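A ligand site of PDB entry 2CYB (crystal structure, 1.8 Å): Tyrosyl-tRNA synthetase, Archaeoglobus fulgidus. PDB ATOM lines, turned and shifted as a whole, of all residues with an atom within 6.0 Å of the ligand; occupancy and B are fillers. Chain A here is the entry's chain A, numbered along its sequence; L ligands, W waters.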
ATOM      1  N   TYR A  36     -19.326   7.450  14.240  1.00  0.00           N
ATOM      2  CA  TYR A  36     -18.551   7.940  15.371  1.00  0.00           C
ATOM      3  C   TYR A  36     -19.343   7.791  16.655  1.00  0.00           C
ATOM      4  O   TYR A  36     -20.527   7.494  16.646  1.00  0.00           O
ATOM      5  CB  TYR A  36     -18.189   9.431  15.206  1.00  0.00           C
ATOM      6  CG  TYR A  36     -19.136  10.430  15.894  1.00  0.00           C
ATOM      7  CD1 TYR A  36     -18.645  11.393  16.773  1.00  0.00           C
ATOM      8  CD2 TYR A  36     -20.514  10.422  15.638  1.00  0.00           C
ATOM      9  CE1 TYR A  36     -19.495  12.333  17.383  1.00  0.00           C
ATOM     10  CE2 TYR A  36     -21.370  11.346  16.234  1.00  0.00           C
ATOM     11  CZ  TYR A  36     -20.862  12.297  17.105  1.00  0.00           C
ATOM     12  OH  TYR A  36     -21.704  13.225  17.677  1.00  0.00           O
ATOM     13  N   VAL A  37     -18.626   8.007  17.750  1.00  0.00           N
ATOM     14  CA  VAL A  37     -19.211   8.031  19.074  1.00  0.00           C
ATOM     15  C   VAL A  37     -18.385   9.118  19.739  1.00  0.00           C
ATOM     16  O   VAL A  37     -17.180   9.249  19.485  1.00  0.00           O
ATOM     17  CB  VAL A  37     -19.033   6.725  19.896  1.00  0.00           C
ATOM     18  CG1 VAL A  37     -19.641   6.933  21.295  1.00  0.00           C
ATOM     19  CG2 VAL A  37     -19.728   5.560  19.204  1.00  0.00           C
ATOM     20  N   GLY A  38     -19.049   9.919  20.558  1.00  0.00           N
ATOM     21  CA  GLY A  38     -18.332  10.974  21.253  1.00  0.00           C
ATOM     22  C   GLY A  38     -18.313  10.617  22.717  1.00  0.00           C
ATOM     23  O   GLY A  38     -19.263  10.028  23.225  1.00  0.00           O
ATOM     24  N   TYR A  39     -17.217  10.962  23.392  1.00  0.00           N
ATOM     25  CA  TYR A  39     -17.096  10.690  24.821  1.00  0.00           C
ATOM     26  C   TYR A  39     -16.550  11.878  25.604  1.00  0.00           C
ATOM     27  O   TYR A  39     -15.556  12.484  25.198  1.00  0.00           O
ATOM     28  CB  TYR A  39     -16.123   9.522  25.070  1.00  0.00           C
ATOM     29  CG  TYR A  39     -16.472   8.212  24.423  1.00  0.00           C
ATOM     30  CD1 TYR A  39     -15.926   7.859  23.179  1.00  0.00           C
ATOM     31  CD2 TYR A  39     -17.302   7.288  25.053  1.00  0.00           C
ATOM     32  CE1 TYR A  39     -16.198   6.625  22.589  1.00  0.00           C
ATOM     33  CE2 TYR A  39     -17.583   6.043  24.472  1.00  0.00           C
ATOM     34  CZ  TYR A  39     -17.018   5.723  23.245  1.00  0.00           C
ATOM     35  OH  TYR A  39     -17.277   4.508  22.657  1.00  0.00           O
ATOM     36  N   GLU A  40     -17.191  12.209  26.715  1.00  0.00           N
ATOM     37  CA  GLU A  40     -16.667  13.279  27.565  1.00  0.00           C
ATOM     38  C   GLU A  40     -15.497  12.568  28.259  1.00  0.00           C
ATOM     39  O   GLU A  40     -15.681  11.512  28.847  1.00  0.00           O
ATOM     40  CB  GLU A  40     -17.678  13.694  28.640  1.00  0.00           C
ATOM     41  CG  GLU A  40     -18.955  14.297  28.147  1.00  0.00           C
ATOM     42  CD  GLU A  40     -19.836  14.766  29.289  1.00  0.00           C
ATOM     43  OE1 GLU A  40     -21.059  14.929  29.078  1.00  0.00           O
ATOM     44  OE2 GLU A  40     -19.312  14.967  30.410  1.00  0.00           O
ATOM     45  N   LEU A  69     -14.599  10.679  19.011  1.00  0.00           N
ATOM     46  CA  LEU A  69     -14.493  12.064  19.456  1.00  0.00           C
ATOM     47  C   LEU A  69     -14.264  12.152  20.957  1.00  0.00           C
ATOM     48  O   LEU A  69     -15.102  11.720  21.754  1.00  0.00           O
ATOM     49  CB  LEU A  69     -15.754  12.860  19.094  1.00  0.00           C
ATOM     50  CG  LEU A  69     -15.831  14.279  19.686  1.00  0.00           C
ATOM     51  CD1 LEU A  69     -14.721  15.143  19.101  1.00  0.00           C
ATOM     52  CD2 LEU A  69     -17.189  14.879  19.376  1.00  0.00           C
ATOM     53  N   ALA A  71     -14.568  14.394  23.392  1.00  0.00           N
ATOM     54  CA  ALA A  71     -15.253  15.668  23.542  1.00  0.00           C
ATOM     55  C   ALA A  71     -14.842  16.458  24.768  1.00  0.00           C
ATOM     56  O   ALA A  71     -15.600  16.566  25.733  1.00  0.00           O
ATOM     57  CB  ALA A  71     -16.779  15.422  23.566  1.00  0.00           C
ATOM     58  N   HIS A  74     -17.145  19.474  25.618  1.00  0.00           N
ATOM     59  CA  HIS A  74     -18.402  18.996  26.189  1.00  0.00           C
ATOM     60  C   HIS A  74     -18.222  18.639  27.663  1.00  0.00           C
ATOM     61  O   HIS A  74     -19.085  18.957  28.495  1.00  0.00           O
ATOM     62  CB  HIS A  74     -18.927  17.781  25.414  1.00  0.00           C
ATOM     63  CG  HIS A  74     -19.642  18.134  24.149  1.00  0.00           C
ATOM     64  ND1 HIS A  74     -18.968  18.429  22.986  1.00  0.00           N
ATOM     65  CD2 HIS A  74     -20.953  18.304  23.887  1.00  0.00           C
ATOM     66  CE1 HIS A  74     -19.849  18.755  22.050  1.00  0.00           C
ATOM     67  NE2 HIS A  74     -21.060  18.689  22.576  1.00  0.00           N
ATOM     68  N   ASN A  78     -20.137  20.297  30.820  1.00  0.00           N
ATOM     69  CA  ASN A  78     -20.917  19.424  31.702  1.00  0.00           C
ATOM     70  C   ASN A  78     -20.276  19.286  33.075  1.00  0.00           C
ATOM     71  O   ASN A  78     -20.447  18.275  33.760  1.00  0.00           O
ATOM     72  CB  ASN A  78     -21.097  18.055  31.044  1.00  0.00           C
ATOM     73  CG  ASN A  78     -22.400  17.353  31.462  1.00  0.00           C
ATOM     74  OD1 ASN A  78     -22.654  16.208  31.078  1.00  0.00           O
ATOM     75  ND2 ASN A  78     -23.207  18.036  32.261  1.00  0.00           N
ATOM     76  N   TYR A 115     -11.570  21.696  16.559  1.00  0.00           N
ATOM     77  CA  TYR A 115     -12.389  22.416  15.599  1.00  0.00           C
ATOM     78  C   TYR A 115     -13.601  23.130  16.193  1.00  0.00           C
ATOM     79  O   TYR A 115     -14.214  23.955  15.535  1.00  0.00           O
ATOM     80  CB  TYR A 115     -12.904  21.443  14.538  1.00  0.00           C
ATOM     81  CG  TYR A 115     -13.838  20.396  15.105  1.00  0.00           C
ATOM     82  CD1 TYR A 115     -13.338  19.230  15.700  1.00  0.00           C
ATOM     83  CD2 TYR A 115     -15.227  20.586  15.099  1.00  0.00           C
ATOM     84  CE1 TYR A 115     -14.201  18.276  16.265  1.00  0.00           C
ATOM     85  CE2 TYR A 115     -16.091  19.644  15.657  1.00  0.00           C
ATOM     86  CZ  TYR A 115     -15.573  18.489  16.239  1.00  0.00           C
ATOM     87  OH  TYR A 115     -16.428  17.559  16.788  1.00  0.00           O
ATOM     88  N   GLN A 116     -13.957  22.821  17.439  1.00  0.00           N
ATOM     89  CA  GLN A 116     -15.141  23.441  18.051  1.00  0.00           C
ATOM     90  C   GLN A 116     -15.017  24.916  18.421  1.00  0.00           C
ATOM     91  O   GLN A 116     -15.983  25.515  18.892  1.00  0.00           O
ATOM     92  CB  GLN A 116     -15.583  22.630  19.271  1.00  0.00           C
ATOM     93  CG  GLN A 116     -16.008  21.231  18.887  1.00  0.00           C
ATOM     94  CD  GLN A 116     -16.276  20.332  20.087  1.00  0.00           C
ATOM     95  OE1 GLN A 116     -15.642  20.458  21.144  1.00  0.00           O
ATOM     96  NE2 GLN A 116     -17.192  19.393  19.914  1.00  0.00           N
ATOM     97  N   VAL A 144     -28.612  13.472  30.213  1.00  0.00           N
ATOM     98  CA  VAL A 144     -27.194  13.695  29.908  1.00  0.00           C
ATOM     99  C   VAL A 144     -26.509  14.708  30.826  1.00  0.00           C
ATOM    100  O   VAL A 144     -25.350  14.509  31.218  1.00  0.00           O
ATOM    101  CB  VAL A 144     -27.043  14.180  28.449  1.00  0.00           C
ATOM    102  CG1 VAL A 144     -25.569  14.410  28.119  1.00  0.00           C
ATOM    103  CG2 VAL A 144     -27.652  13.160  27.508  1.00  0.00           C
ATOM    104  N   TYR A 158     -24.472  22.629  25.064  1.00  0.00           N
ATOM    105  CA  TYR A 158     -23.980  21.257  24.893  1.00  0.00           C
ATOM    106  C   TYR A 158     -24.685  20.423  23.787  1.00  0.00           C
ATOM    107  O   TYR A 158     -24.019  19.894  22.889  1.00  0.00           O
ATOM    108  CB  TYR A 158     -24.075  20.557  26.259  1.00  0.00           C
ATOM    109  CG  TYR A 158     -23.542  19.143  26.378  1.00  0.00           C
ATOM    110  CD1 TYR A 158     -22.481  18.835  27.249  1.00  0.00           C
ATOM    111  CD2 TYR A 158     -24.142  18.098  25.686  1.00  0.00           C
ATOM    112  CE1 TYR A 158     -22.057  17.519  27.428  1.00  0.00           C
ATOM    113  CE2 TYR A 158     -23.724  16.788  25.847  1.00  0.00           C
ATOM    114  CZ  TYR A 158     -22.683  16.506  26.709  1.00  0.00           C
ATOM    115  OH  TYR A 158     -22.262  15.203  26.839  1.00  0.00           O
ATOM    116  N   MET A 161     -23.991  21.633  20.177  1.00  0.00           N
ATOM    117  CA  MET A 161     -22.643  21.305  19.741  1.00  0.00           C
ATOM    118  C   MET A 161     -22.520  19.834  19.390  1.00  0.00           C
ATOM    119  O   MET A 161     -21.801  19.491  18.472  1.00  0.00           O
ATOM    120  CB  MET A 161     -21.634  21.685  20.818  1.00  0.00           C
ATOM    121  CG  MET A 161     -21.370  23.186  20.877  1.00  0.00           C
ATOM    122  SD  MET A 161     -20.155  23.586  22.142  1.00  0.00           S
ATOM    123  CE  MET A 161     -18.731  22.611  21.604  1.00  0.00           C
ATOM    124  N   GLN A 162     -23.203  18.968  20.140  1.00  0.00           N
ATOM    125  CA  GLN A 162     -23.145  17.550  19.835  1.00  0.00           C
ATOM    126  C   GLN A 162     -23.742  17.306  18.450  1.00  0.00           C
ATOM    127  O   GLN A 162     -23.182  16.571  17.647  1.00  0.00           O
ATOM    128  CB  GLN A 162     -23.924  16.739  20.877  1.00  0.00           C
ATOM    129  CG  GLN A 162     -23.858  15.243  20.621  1.00  0.00           C
ATOM    130  CD  GLN A 162     -24.306  14.437  21.823  1.00  0.00           C
ATOM    131  OE1 GLN A 162     -24.163  14.878  22.960  1.00  0.00           O
ATOM    132  NE2 GLN A 162     -24.818  13.228  21.576  1.00  0.00           N
ATOM    133  N   ALA A 163     -24.883  17.939  18.189  1.00  0.00           N
ATOM    134  CA  ALA A 163     -25.538  17.796  16.894  1.00  0.00           C
ATOM    135  C   ALA A 163     -24.594  18.299  15.799  1.00  0.00           C
ATOM    136  O   ALA A 163     -24.463  17.671  14.756  1.00  0.00           O
ATOM    137  CB  ALA A 163     -26.845  18.585  16.868  1.00  0.00           C
ATOM    138  N   ASP A 165     -21.393  18.347  15.863  1.00  0.00           N
ATOM    139  CA  ASP A 165     -20.226  17.490  15.723  1.00  0.00           C
ATOM    140  C   ASP A 165     -20.470  16.476  14.598  1.00  0.00           C
ATOM    141  O   ASP A 165     -19.551  16.124  13.860  1.00  0.00           O
ATOM    142  CB  ASP A 165     -19.928  16.730  17.018  1.00  0.00           C
ATOM    143  CG  ASP A 165     -19.412  17.622  18.107  1.00  0.00           C
ATOM    144  OD1 ASP A 165     -19.565  17.256  19.279  1.00  0.00           O
ATOM    145  OD2 ASP A 165     -18.833  18.688  17.783  1.00  0.00           O
ATOM    146  N   ILE A 166     -21.712  16.020  14.480  1.00  0.00           N
ATOM    147  CA  ILE A 166     -22.069  15.040  13.461  1.00  0.00           C
ATOM    148  C   ILE A 166     -21.774  15.618  12.067  1.00  0.00           C
ATOM    149  O   ILE A 166     -21.119  14.980  11.236  1.00  0.00           O
ATOM    150  CB  ILE A 166     -23.567  14.668  13.547  1.00  0.00           C
ATOM    151  CG1 ILE A 166     -23.840  13.918  14.859  1.00  0.00           C
ATOM    152  CG2 ILE A 166     -23.964  13.802  12.358  1.00  0.00           C
ATOM    153  CD1 ILE A 166     -25.310  13.763  15.179  1.00  0.00           C
ATOM    154  N   LEU A 169     -17.841  16.545  11.502  1.00  0.00           N
ATOM    155  CA  LEU A 169     -16.937  15.393  11.418  1.00  0.00           C
ATOM    156  C   LEU A 169     -17.292  14.542  10.189  1.00  0.00           C
ATOM    157  O   LEU A 169     -16.705  13.483   9.960  1.00  0.00           O
ATOM    158  CB  LEU A 169     -17.030  14.548  12.695  1.00  0.00           C
ATOM    159  CG  LEU A 169     -16.500  15.211  13.969  1.00  0.00           C
ATOM    160  CD1 LEU A 169     -16.893  14.370  15.188  1.00  0.00           C
ATOM    161  CD2 LEU A 169     -14.988  15.379  13.891  1.00  0.00           C
ATOM    162  N   ASP A 179     -29.747   7.071  25.611  1.00  0.00           N
ATOM    163  CA  ASP A 179     -29.980   8.315  26.332  1.00  0.00           C
ATOM    164  C   ASP A 179     -29.568   9.541  25.508  1.00  0.00           C
ATOM    165  O   ASP A 179     -29.788  10.676  25.921  1.00  0.00           O
ATOM    166  CB  ASP A 179     -29.285   8.316  27.701  1.00  0.00           C
ATOM    167  CG  ASP A 179     -27.811   7.944  27.628  1.00  0.00           C
ATOM    168  OD1 ASP A 179     -27.289   7.629  26.533  1.00  0.00           O
ATOM    169  OD2 ASP A 179     -27.170   7.968  28.705  1.00  0.00           O
ATOM    170  N   GLN A 180     -28.989   9.288  24.341  1.00  0.00           N
ATOM    171  CA  GLN A 180     -28.569  10.385  23.443  1.00  0.00           C
ATOM    172  C   GLN A 180     -29.681  10.590  22.403  1.00  0.00           C
ATOM    173  O   GLN A 180     -29.563  11.442  21.521  1.00  0.00           O
ATOM    174  CB  GLN A 180     -27.291  10.029  22.682  1.00  0.00           C
ATOM    175  CG  GLN A 180     -26.110   9.578  23.540  1.00  0.00           C
ATOM    176  CD  GLN A 180     -25.723  10.601  24.575  1.00  0.00           C
ATOM    177  OE1 GLN A 180     -25.452  11.763  24.246  1.00  0.00           O
ATOM    178  NE2 GLN A 180     -25.697  10.190  25.836  1.00  0.00           N
ATOM    179  N   ILE A 183     -31.072  14.189  21.714  1.00  0.00           N
ATOM    180  CA  ILE A 183     -30.071  15.031  21.087  1.00  0.00           C
ATOM    181  C   ILE A 183     -29.975  14.627  19.615  1.00  0.00           C
ATOM    182  O   ILE A 183     -29.922  15.470  18.727  1.00  0.00           O
ATOM    183  CB  ILE A 183     -28.700  14.905  21.778  1.00  0.00           C
ATOM    184  CG1 ILE A 183     -28.765  15.544  23.174  1.00  0.00           C
ATOM    185  CG2 ILE A 183     -27.623  15.570  20.935  1.00  0.00           C
ATOM    186  CD1 ILE A 183     -27.493  15.367  24.006  1.00  0.00           C
HETATM  187  N1  LIG L   1     -23.348  13.273  25.052  1.00  0.00           N
HETATM  188  C1  LIG L   1     -22.420  12.119  25.080  1.00  0.00           C
HETATM  189  C2  LIG L   1     -22.486  11.380  26.415  1.00  0.00           C
HETATM  190  O1  LIG L   1     -21.756  10.395  26.570  1.00  0.00           O
HETATM  191  C3  LIG L   1     -20.987  12.613  24.811  1.00  0.00           C
HETATM  192  C4  LIG L   1     -20.860  13.225  23.441  1.00  0.00           C
HETATM  193  C5  LIG L   1     -20.401  14.534  23.269  1.00  0.00           C
HETATM  194  C6  LIG L   1     -21.220  12.499  22.296  1.00  0.00           C
HETATM  195  C7  LIG L   1     -20.293  15.104  21.989  1.00  0.00           C
HETATM  196  C8  LIG L   1     -21.110  13.045  21.030  1.00  0.00           C
HETATM  197  C9  LIG L   1     -20.646  14.347  20.876  1.00  0.00           C
HETATM  198  O2  LIG L   1     -20.526  14.858  19.617  1.00  0.00           O
HETATM  199  O3  LIG L   1     -23.286  11.803  27.283  1.00  0.00           O
HETATM  200  O   HOH W   1     -22.871   8.773  28.522  1.00  0.00           O
HETATM  201  O   HOH W   2     -20.346   8.436  25.242  1.00  0.00           O
HETATM  202  O   HOH W   3     -19.301  10.724  27.725  1.00  0.00           O
HETATM  203  O   HOH W   4     -22.396   9.320  23.035  1.00  0.00           O
HETATM  204  O   HOH W   5     -23.641  11.791  19.175  1.00  0.00           O
HETATM  205  O   HOH W   6     -25.336  10.572  29.319  1.00  0.00           O
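OD2 of Asp 165 is in hydrogen-bond range of NE2 of Gln 116 (2.8 Å). The side-chain hydroxyl (OH) of Tyr 115 lies within hydrogen-bond range of the side-chain carboxylate (OD2) of Asp 165. OE1 of Gln 180 sits at hydrogen-bond distance from NE2 of Gln 162, at 3.1 Å. OD1 of Asp 179 sits at hydrogen-bond distance from NE2 of Gln 180 (3.1 Å). The backbone carbonyl oxygen of Tyr 158 lies within hydrogen-bond range of a ring nitrogen (NE2) of His 74, 3.2 Å away. O of Leu 69 lies within hydrogen-bond range of N of Tyr 39, 2.8 Å away. The backbone NH of Leu 69 is in hydrogen-bond range of the backbone carbonyl oxygen of Val 37 (3.0 Å). OD1 of Asn 78 lies close to O of Val 144, at 3.2 Å.
Water W3 bridges an oxygen (O1) of the ligand (2.7 Å) and the backbone NH of Glu 40 (2.8 Å). Water W2 lies within hydrogen-bond range of O1 of the ligand and O of Gly 38. Water W6 lies within hydrogen-bond range of an oxygen (O3) of the ligand (3.1 Å) and the side-chain carboxylate of Asp 179 (3.2 Å). Water W5 bridges OH of Tyr 36 and NE2 of Gln 162.
An oxygen (O2) of the ligand is in hydrogen-bond range of the side-chain carboxylate of Asp 165 (2.6 Å). The side-chain amide oxygen (OE1) of Gln 180 lies within hydrogen-bond range of a nitrogen (N1) of the ligand. The side-chain amide oxygen of Gln 162 sits at hydrogen-bond distance from a nitrogen (N1) of the ligand. O2 of the ligand is in hydrogen-bond range of OH of Tyr 36 (2.8 Å). A nitrogen (N1) of the ligand sits at hydrogen-bond distance from the side-chain hydroxyl of Tyr 158, at 2.8 Å.
Gly 38 touches the ligand. Leu 69 touches the ligand (CD2 to O2, 3.3 Å). Ala 71 touches the ligand. His 74 touches the ligand. CG1 of Val 144 touches O3 of the ligand, 3.6 Å away. Hydrophobic or aromatic side chains that line the ligand: Tyr 36, Leu 69, Ala 71, His 74, Val 144 and Tyr 158. Within 4 Å of the ligand: Tyr 36, Gly 38, Leu 69, Ala 71, His 74, Val 144, Tyr 158, Gln 162, Asp 165 and Gln 180. Along chain A the residues within 4 Å of the ligand span positions 36 to 180.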
